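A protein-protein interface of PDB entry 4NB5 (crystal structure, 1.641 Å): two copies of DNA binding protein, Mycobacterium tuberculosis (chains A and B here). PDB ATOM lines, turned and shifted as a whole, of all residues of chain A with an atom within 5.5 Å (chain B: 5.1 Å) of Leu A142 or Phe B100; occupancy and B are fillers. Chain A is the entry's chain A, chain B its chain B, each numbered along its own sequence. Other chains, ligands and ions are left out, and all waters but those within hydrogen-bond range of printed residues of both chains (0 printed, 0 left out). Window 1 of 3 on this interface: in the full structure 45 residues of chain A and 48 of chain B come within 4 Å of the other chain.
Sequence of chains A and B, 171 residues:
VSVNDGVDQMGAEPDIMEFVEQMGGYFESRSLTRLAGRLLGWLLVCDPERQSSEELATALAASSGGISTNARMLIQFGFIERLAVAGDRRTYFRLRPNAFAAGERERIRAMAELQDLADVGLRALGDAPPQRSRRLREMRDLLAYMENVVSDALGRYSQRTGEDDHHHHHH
OE2 of Glu A138 sits close to OD1 of Asn B98 (2.6 Å).
The side-chain carboxylate (OE1) of Glu A138 is in hydrogen-bond range of the backbone NH (N) of Ala B99.
The side-chain carboxylate of Glu A138 is in hydrogen-bond range of the backbone NH of Phe B100, 3.1 Å away.
OH of Tyr B157 is in hydrogen-bond range of N of Leu A142, at 3.3 Å.
Among the printed residues, merely in contact across the chains: Asp A141 with Tyr B157, Tyr A145 with Tyr B157, Met A139 with Phe B100, Leu A142 with Phe B100, Leu A142 with Ala B101, Glu A138 with Ala B101, Leu A114 with Phe B100 and Met A139 with Leu B44.
Of chain B, only Phe B100 (3.6 Å), Ala B101 (3.7 Å) and Tyr B157 (3.3 Å) come within 4 Å of Leu A142.
Of the printed residues of chain A, Tyr B157 touches Asp A141 (3.3 Å), Leu A142 (3.3 Å) and Tyr A145 (3.5 Å).
Of the printed residues of chain B, Glu A138 touches Asn B98 (2.6 Å), Ala B99 (3.4 Å), Phe B100 (3.1 Å) and Ala B101 (3.7 Å).
Of the printed residues of chain B, Tyr A145 touches Tyr B157.
Printed residues of chain B within 4 Å of Leu A114: Phe B100 (3.7 Å).
Of the printed residues of chain A, Ala B101 touches Glu A138 (3.7 Å) and Leu A142 (3.7 Å).
Arg A137 touches none of the printed residues of chain B.
The nearest residue of chain B that does not touch Leu A142 is Glu B104 (4.02 Å).
The nearest printed residue of chain A that does not touch Phe B100 is Leu A143 (4.3 Å).
The nearest printed residue of chain B that does not touch Tyr A145 is Leu B154 (4.8 Å).
Of the 12 printed residues of chain A, 6 touch a printed residue of chain B.
Hydrophobic or aromatic side chains of chain A that line the printed part of chain B: Leu A114, Met A139, Leu A142 and Tyr A145.
Along chain A the printed residues that touch a printed residue of chain B span positions 114 to 145.
Hydrophobic or aromatic side chains of chain B within 4 Å of the printed part of chain A: Leu B44, Phe B100 and Tyr B157.
Along chain B the printed residues that touch a printed residue of chain A span positions 44 to 157.
No position is printed for both chains.
Of the 12 pairs that touch across the chains among the printed residues, none has its exchanged pair printed and touching as well.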
ATOM      1  N   LEU A 114      12.487 -13.432  31.860  1.00  0.00           N
ATOM      2  CA  LEU A 114      12.504 -11.993  32.048  1.00  0.00           C
ATOM      3  C   LEU A 114      11.637 -11.296  30.994  1.00  0.00           C
ATOM      4  O   LEU A 114      10.940 -10.318  31.274  1.00  0.00           O
ATOM      5  CB  LEU A 114      13.945 -11.495  31.981  1.00  0.00           C
ATOM      6  CG  LEU A 114      14.170 -10.054  32.422  1.00  0.00           C
ATOM      7  CD1 LEU A 114      13.635  -9.821  33.836  1.00  0.00           C
ATOM      8  CD2 LEU A 114      15.640  -9.722  32.357  1.00  0.00           C
ATOM      9  N   ARG A 137       9.061  -1.997  26.027  1.00  0.00           N
ATOM     10  CA  ARG A 137       9.141  -2.486  24.653  1.00  0.00           C
ATOM     11  C   ARG A 137      10.595  -2.722  24.235  1.00  0.00           C
ATOM     12  O   ARG A 137      10.889  -3.742  23.615  1.00  0.00           O
ATOM     13  CB  ARG A 137       8.433  -1.539  23.672  1.00  0.00           C
ATOM     14  CG  ARG A 137       6.912  -1.652  23.704  1.00  0.00           C
ATOM     15  CD  ARG A 137       6.270  -0.942  22.508  1.00  0.00           C
ATOM     16  NE  ARG A 137       6.795   0.413  22.338  1.00  0.00           N
ATOM     17  CZ  ARG A 137       6.242   1.510  22.856  1.00  0.00           C
ATOM     18  NH1 ARG A 137       5.134   1.437  23.585  1.00  0.00           N
ATOM     19  NH2 ARG A 137       6.802   2.694  22.644  1.00  0.00           N
ATOM     20  N   GLU A 138      11.492  -1.794  24.587  1.00  0.00           N
ATOM     21  CA  GLU A 138      12.934  -1.941  24.309  1.00  0.00           C
ATOM     22  C   GLU A 138      13.471  -3.185  24.974  1.00  0.00           C
ATOM     23  O   GLU A 138      14.235  -3.945  24.372  1.00  0.00           O
ATOM     24  CB  GLU A 138      13.732  -0.753  24.883  1.00  0.00           C
ATOM     25  CG  GLU A 138      15.262  -0.679  24.548  1.00  0.00           C
ATOM     26  CD  GLU A 138      16.206  -1.720  25.232  1.00  0.00           C
ATOM     27  OE1 GLU A 138      16.116  -2.036  26.456  1.00  0.00           O
ATOM     28  OE2 GLU A 138      17.112  -2.191  24.510  1.00  0.00           O
ATOM     29  N   MET A 139      13.080  -3.381  26.231  1.00  0.00           N
ATOM     30  CA  MET A 139      13.516  -4.521  27.030  1.00  0.00           C
ATOM     31  C   MET A 139      13.087  -5.822  26.363  1.00  0.00           C
ATOM     32  O   MET A 139      13.904  -6.728  26.129  1.00  0.00           O
ATOM     33  CB  MET A 139      12.909  -4.430  28.429  1.00  0.00           C
ATOM     34  CG  MET A 139      13.048  -5.672  29.278  1.00  0.00           C
ATOM     35  SD  MET A 139      12.203  -5.427  30.854  1.00  0.00           S
ATOM     36  CE  MET A 139      12.536  -6.982  31.690  1.00  0.00           C
ATOM     37  N   ARG A 140      11.799  -5.912  26.056  1.00  0.00           N
ATOM     38  CA  ARG A 140      11.256  -7.106  25.411  1.00  0.00           C
ATOM     39  C   ARG A 140      11.928  -7.386  24.066  1.00  0.00           C
ATOM     40  O   ARG A 140      12.285  -8.529  23.764  1.00  0.00           O
ATOM     41  CB  ARG A 140       9.741  -6.961  25.215  1.00  0.00           C
ATOM     42  CG  ARG A 140       9.111  -8.189  24.566  1.00  0.00           C
ATOM     43  CD  ARG A 140       7.612  -8.094  24.489  1.00  0.00           C
ATOM     44  NE  ARG A 140       7.166  -7.005  23.640  1.00  0.00           N
ATOM     45  CZ  ARG A 140       5.887  -6.763  23.359  1.00  0.00           C
ATOM     46  NH1 ARG A 140       4.936  -7.545  23.856  1.00  0.00           N
ATOM     47  NH2 ARG A 140       5.567  -5.750  22.576  1.00  0.00           N
ATOM     48  N   ASP A 141      12.089  -6.342  23.255  1.00  0.00           N
ATOM     49  CA  ASP A 141      12.660  -6.486  21.917  1.00  0.00           C
ATOM     50  C   ASP A 141      14.105  -7.005  21.996  1.00  0.00           C
ATOM     51  O   ASP A 141      14.499  -7.901  21.260  1.00  0.00           O
ATOM     52  CB  ASP A 141      12.614  -5.148  21.179  1.00  0.00           C
ATOM     53  CG  ASP A 141      11.202  -4.727  20.820  1.00  0.00           C
ATOM     54  OD1 ASP A 141      10.283  -5.562  20.948  1.00  0.00           O
ATOM     55  OD2 ASP A 141      11.015  -3.568  20.395  1.00  0.00           O
ATOM     56  N   LEU A 142      14.880  -6.447  22.914  1.00  0.00           N
ATOM     57  CA  LEU A 142      16.285  -6.822  23.039  1.00  0.00           C
ATOM     58  C   LEU A 142      16.427  -8.253  23.527  1.00  0.00           C
ATOM     59  O   LEU A 142      17.212  -9.027  22.982  1.00  0.00           O
ATOM     60  CB  LEU A 142      16.998  -5.854  23.976  1.00  0.00           C
ATOM     61  CG  LEU A 142      18.508  -6.025  24.185  1.00  0.00           C
ATOM     62  CD1 LEU A 142      18.827  -7.170  25.119  1.00  0.00           C
ATOM     63  CD2 LEU A 142      19.210  -6.212  22.848  1.00  0.00           C
ATOM     64  N   LEU A 143      15.660  -8.604  24.555  1.00  0.00           N
ATOM     65  CA  LEU A 143      15.713  -9.953  25.094  1.00  0.00           C
ATOM     66  C   LEU A 143      15.368 -10.993  24.026  1.00  0.00           C
ATOM     67  O   LEU A 143      16.062 -12.004  23.884  1.00  0.00           O
ATOM     68  CB  LEU A 143      14.795 -10.095  26.317  1.00  0.00           C
ATOM     69  CG  LEU A 143      15.236  -9.283  27.541  1.00  0.00           C
ATOM     70  CD1 LEU A 143      14.132  -9.286  28.600  1.00  0.00           C
ATOM     71  CD2 LEU A 143      16.538  -9.842  28.122  1.00  0.00           C
ATOM     72  N   ALA A 144      14.297 -10.756  23.276  1.00  0.00           N
ATOM     73  CA  ALA A 144      13.937 -11.661  22.188  1.00  0.00           C
ATOM     74  C   ALA A 144      15.083 -11.802  21.183  1.00  0.00           C
ATOM     75  O   ALA A 144      15.441 -12.912  20.770  1.00  0.00           O
ATOM     76  CB  ALA A 144      12.682 -11.154  21.483  1.00  0.00           C
ATOM     77  N   TYR A 145      15.652 -10.671  20.786  1.00  0.00           N
ATOM     78  CA  TYR A 145      16.714 -10.654  19.792  1.00  0.00           C
ATOM     79  C   TYR A 145      17.903 -11.460  20.292  1.00  0.00           C
ATOM     80  O   TYR A 145      18.432 -12.315  19.580  1.00  0.00           O
ATOM     81  CB  TYR A 145      17.122  -9.217  19.524  1.00  0.00           C
ATOM     82  CG  TYR A 145      18.226  -9.053  18.502  1.00  0.00           C
ATOM     83  CD1 TYR A 145      17.950  -9.084  17.144  1.00  0.00           C
ATOM     84  CD2 TYR A 145      19.530  -8.837  18.904  1.00  0.00           C
ATOM     85  CE1 TYR A 145      18.951  -8.922  16.211  1.00  0.00           C
ATOM     86  CE2 TYR A 145      20.537  -8.664  17.976  1.00  0.00           C
ATOM     87  CZ  TYR A 145      20.242  -8.714  16.634  1.00  0.00           C
ATOM     88  OH  TYR A 145      21.247  -8.549  15.710  1.00  0.00           O
ATOM     89  N   MET A 146      18.317 -11.198  21.528  1.00  0.00           N
ATOM     90  CA  MET A 146      19.463 -11.910  22.096  1.00  0.00           C
ATOM     91  C   MET A 146      19.202 -13.400  22.317  1.00  0.00           C
ATOM     92  O   MET A 146      20.096 -14.216  22.112  1.00  0.00           O
ATOM     93  CB  MET A 146      19.900 -11.243  23.400  1.00  0.00           C
ATOM     94  CG  MET A 146      20.504  -9.872  23.189  1.00  0.00           C
ATOM     95  SD  MET A 146      21.866  -9.819  21.974  1.00  0.00           S
ATOM     96  CE  MET A 146      22.865 -11.156  22.579  1.00  0.00           C
ATOM     97  N   GLU A 147      17.991 -13.757  22.736  1.00  0.00           N
ATOM     98  CA  GLU A 147      17.635 -15.165  22.873  1.00  0.00           C
ATOM     99  C   GLU A 147      17.822 -15.887  21.544  1.00  0.00           C
ATOM    100  O   GLU A 147      18.370 -16.981  21.495  1.00  0.00           O
ATOM    101  CB  GLU A 147      16.187 -15.315  23.324  1.00  0.00           C
ATOM    102  CG  GLU A 147      15.958 -15.054  24.798  1.00  0.00           C
ATOM    103  CD  GLU A 147      14.491 -14.891  25.115  1.00  0.00           C
ATOM    104  OE1 GLU A 147      13.693 -15.798  24.769  1.00  0.00           O
ATOM    105  OE2 GLU A 147      14.122 -13.831  25.662  1.00  0.00           O
ATOM    106  N   LEU B  40      14.790  -1.987  39.666  1.00  0.00           N
ATOM    107  CA  LEU B  40      14.846  -2.039  38.213  1.00  0.00           C
ATOM    108  C   LEU B  40      13.431  -2.051  37.643  1.00  0.00           C
ATOM    109  O   LEU B  40      13.128  -1.335  36.696  1.00  0.00           O
ATOM    110  CB  LEU B  40      15.628  -3.264  37.746  1.00  0.00           C
ATOM    111  CG  LEU B  40      15.735  -3.445  36.228  1.00  0.00           C
ATOM    112  CD1 LEU B  40      16.334  -2.219  35.557  1.00  0.00           C
ATOM    113  CD2 LEU B  40      16.546  -4.679  35.882  1.00  0.00           C
ATOM    114  N   LEU B  44      11.529   0.833  35.204  1.00  0.00           N
ATOM    115  CA  LEU B  44      10.988   0.440  33.911  1.00  0.00           C
ATOM    116  C   LEU B  44       9.567   0.957  33.665  1.00  0.00           C
ATOM    117  O   LEU B  44       9.140   1.056  32.523  1.00  0.00           O
ATOM    118  CB  LEU B  44      10.986  -1.086  33.796  1.00  0.00           C
ATOM    119  CG  LEU B  44      12.320  -1.647  33.323  1.00  0.00           C
ATOM    120  CD1 LEU B  44      12.483  -3.077  33.785  1.00  0.00           C
ATOM    121  CD2 LEU B  44      12.439  -1.585  31.826  1.00  0.00           C
ATOM    122  N   PHE B  79      22.287  -0.927  33.652  1.00  0.00           N
ATOM    123  CA  PHE B  79      20.869  -0.696  33.374  1.00  0.00           C
ATOM    124  C   PHE B  79      20.387   0.720  33.652  1.00  0.00           C
ATOM    125  O   PHE B  79      19.499   1.212  32.955  1.00  0.00           O
ATOM    126  CB  PHE B  79      19.981  -1.657  34.176  1.00  0.00           C
ATOM    127  CG  PHE B  79      20.154  -3.105  33.809  1.00  0.00           C
ATOM    128  CD1 PHE B  79      19.849  -3.552  32.536  1.00  0.00           C
ATOM    129  CD2 PHE B  79      20.599  -4.022  34.747  1.00  0.00           C
ATOM    130  CE1 PHE B  79      20.006  -4.886  32.196  1.00  0.00           C
ATOM    131  CE2 PHE B  79      20.752  -5.358  34.413  1.00  0.00           C
ATOM    132  CZ  PHE B  79      20.453  -5.786  33.131  1.00  0.00           C
ATOM    133  N   ASN B  98      17.906   2.390  25.937  1.00  0.00           N
ATOM    134  CA  ASN B  98      18.315   1.090  25.427  1.00  0.00           C
ATOM    135  C   ASN B  98      18.972   0.265  26.545  1.00  0.00           C
ATOM    136  O   ASN B  98      20.021  -0.354  26.341  1.00  0.00           O
ATOM    137  CB  ASN B  98      19.293   1.310  24.268  1.00  0.00           C
ATOM    138  CG  ASN B  98      19.188   0.249  23.188  1.00  0.00           C
ATOM    139  OD1 ASN B  98      18.149  -0.388  23.019  1.00  0.00           O
ATOM    140  ND2 ASN B  98      20.272   0.064  22.440  1.00  0.00           N
ATOM    141  N   ALA B  99      18.338   0.244  27.719  1.00  0.00           N
ATOM    142  CA  ALA B  99      18.964  -0.276  28.938  1.00  0.00           C
ATOM    143  C   ALA B  99      19.437  -1.720  28.857  1.00  0.00           C
ATOM    144  O   ALA B  99      20.494  -2.057  29.383  1.00  0.00           O
ATOM    145  CB  ALA B  99      18.025  -0.113  30.127  1.00  0.00           C
ATOM    146  N   PHE B 100      18.656  -2.586  28.222  1.00  0.00           N
ATOM    147  CA  PHE B 100      19.025  -3.992  28.192  1.00  0.00           C
ATOM    148  C   PHE B 100      20.118  -4.270  27.151  1.00  0.00           C
ATOM    149  O   PHE B 100      20.912  -5.199  27.308  1.00  0.00           O
ATOM    150  CB  PHE B 100      17.780  -4.873  28.062  1.00  0.00           C
ATOM    151  CG  PHE B 100      17.050  -5.010  29.361  1.00  0.00           C
ATOM    152  CD1 PHE B 100      16.268  -3.966  29.827  1.00  0.00           C
ATOM    153  CD2 PHE B 100      17.204  -6.129  30.157  1.00  0.00           C
ATOM    154  CE1 PHE B 100      15.623  -4.057  31.048  1.00  0.00           C
ATOM    155  CE2 PHE B 100      16.560  -6.224  31.379  1.00  0.00           C
ATOM    156  CZ  PHE B 100      15.767  -5.181  31.819  1.00  0.00           C
ATOM    157  N   ALA B 101      20.201  -3.430  26.131  1.00  0.00           N
ATOM    158  CA  ALA B 101      21.329  -3.497  25.210  1.00  0.00           C
ATOM    159  C   ALA B 101      22.584  -3.060  25.950  1.00  0.00           C
ATOM    160  O   ALA B 101      23.644  -3.671  25.814  1.00  0.00           O
ATOM    161  CB  ALA B 101      21.107  -2.631  24.013  1.00  0.00           C
ATOM    162  N   ALA B 102      22.462  -2.004  26.744  1.00  0.00           N
ATOM    163  CA  ALA B 102      23.582  -1.542  27.563  1.00  0.00           C
ATOM    164  C   ALA B 102      24.001  -2.616  28.572  1.00  0.00           C
ATOM    165  O   ALA B 102      25.192  -2.849  28.816  1.00  0.00           O
ATOM    166  CB  ALA B 102      23.208  -0.254  28.278  1.00  0.00           C
ATOM    167  N   GLY B 103      23.017  -3.286  29.148  1.00  0.00           N
ATOM    168  CA  GLY B 103      23.282  -4.405  30.035  1.00  0.00           C
ATOM    169  C   GLY B 103      24.050  -5.516  29.332  1.00  0.00           C
ATOM    170  O   GLY B 103      25.001  -6.092  29.892  1.00  0.00           O
ATOM    171  N   GLU B 104      23.649  -5.825  28.104  1.00  0.00           N
ATOM    172  CA  GLU B 104      24.347  -6.855  27.340  1.00  0.00           C
ATOM    173  C   GLU B 104      25.775  -6.448  26.995  1.00  0.00           C
ATOM    174  O   GLU B 104      26.658  -7.299  26.902  1.00  0.00           O
ATOM    175  CB  GLU B 104      23.586  -7.217  26.070  1.00  0.00           C
ATOM    176  CG  GLU B 104      22.520  -8.277  26.272  1.00  0.00           C
ATOM    177  CD  GLU B 104      23.078  -9.578  26.834  1.00  0.00           C
ATOM    178  OE1 GLU B 104      22.494 -10.087  27.810  1.00  0.00           O
ATOM    179  OE2 GLU B 104      24.092 -10.084  26.304  1.00  0.00           O
ATOM    180  N   LEU B 154      24.968  -6.972  18.746  1.00  0.00           N
ATOM    181  CA  LEU B 154      24.539  -5.686  19.291  1.00  0.00           C
ATOM    182  C   LEU B 154      24.820  -4.567  18.285  1.00  0.00           C
ATOM    183  O   LEU B 154      24.063  -3.606  18.182  1.00  0.00           O
ATOM    184  CB  LEU B 154      25.228  -5.394  20.623  1.00  0.00           C
ATOM    185  CG  LEU B 154      24.805  -6.253  21.821  1.00  0.00           C
ATOM    186  CD1 LEU B 154      25.650  -5.911  23.030  1.00  0.00           C
ATOM    187  CD2 LEU B 154      23.326  -6.061  22.155  1.00  0.00           C
ATOM    188  N   TYR B 157      22.035  -4.832  15.950  1.00  0.00           N
ATOM    189  CA  TYR B 157      20.789  -4.445  16.601  1.00  0.00           C
ATOM    190  C   TYR B 157      20.585  -2.927  16.538  1.00  0.00           C
ATOM    191  O   TYR B 157      19.476  -2.449  16.311  1.00  0.00           O
ATOM    192  CB  TYR B 157      20.779  -4.925  18.054  1.00  0.00           C
ATOM    193  CG  TYR B 157      19.443  -4.762  18.728  1.00  0.00           C
ATOM    194  CD1 TYR B 157      18.372  -5.561  18.365  1.00  0.00           C
ATOM    195  CD2 TYR B 157      19.251  -3.810  19.718  1.00  0.00           C
ATOM    196  CE1 TYR B 157      17.148  -5.426  18.968  1.00  0.00           C
ATOM    197  CE2 TYR B 157      18.014  -3.662  20.330  1.00  0.00           C
ATOM    198  CZ  TYR B 157      16.973  -4.481  19.946  1.00  0.00           C
ATOM    199  OH  TYR B 157      15.740  -4.358  20.531  1.00  0.00           O
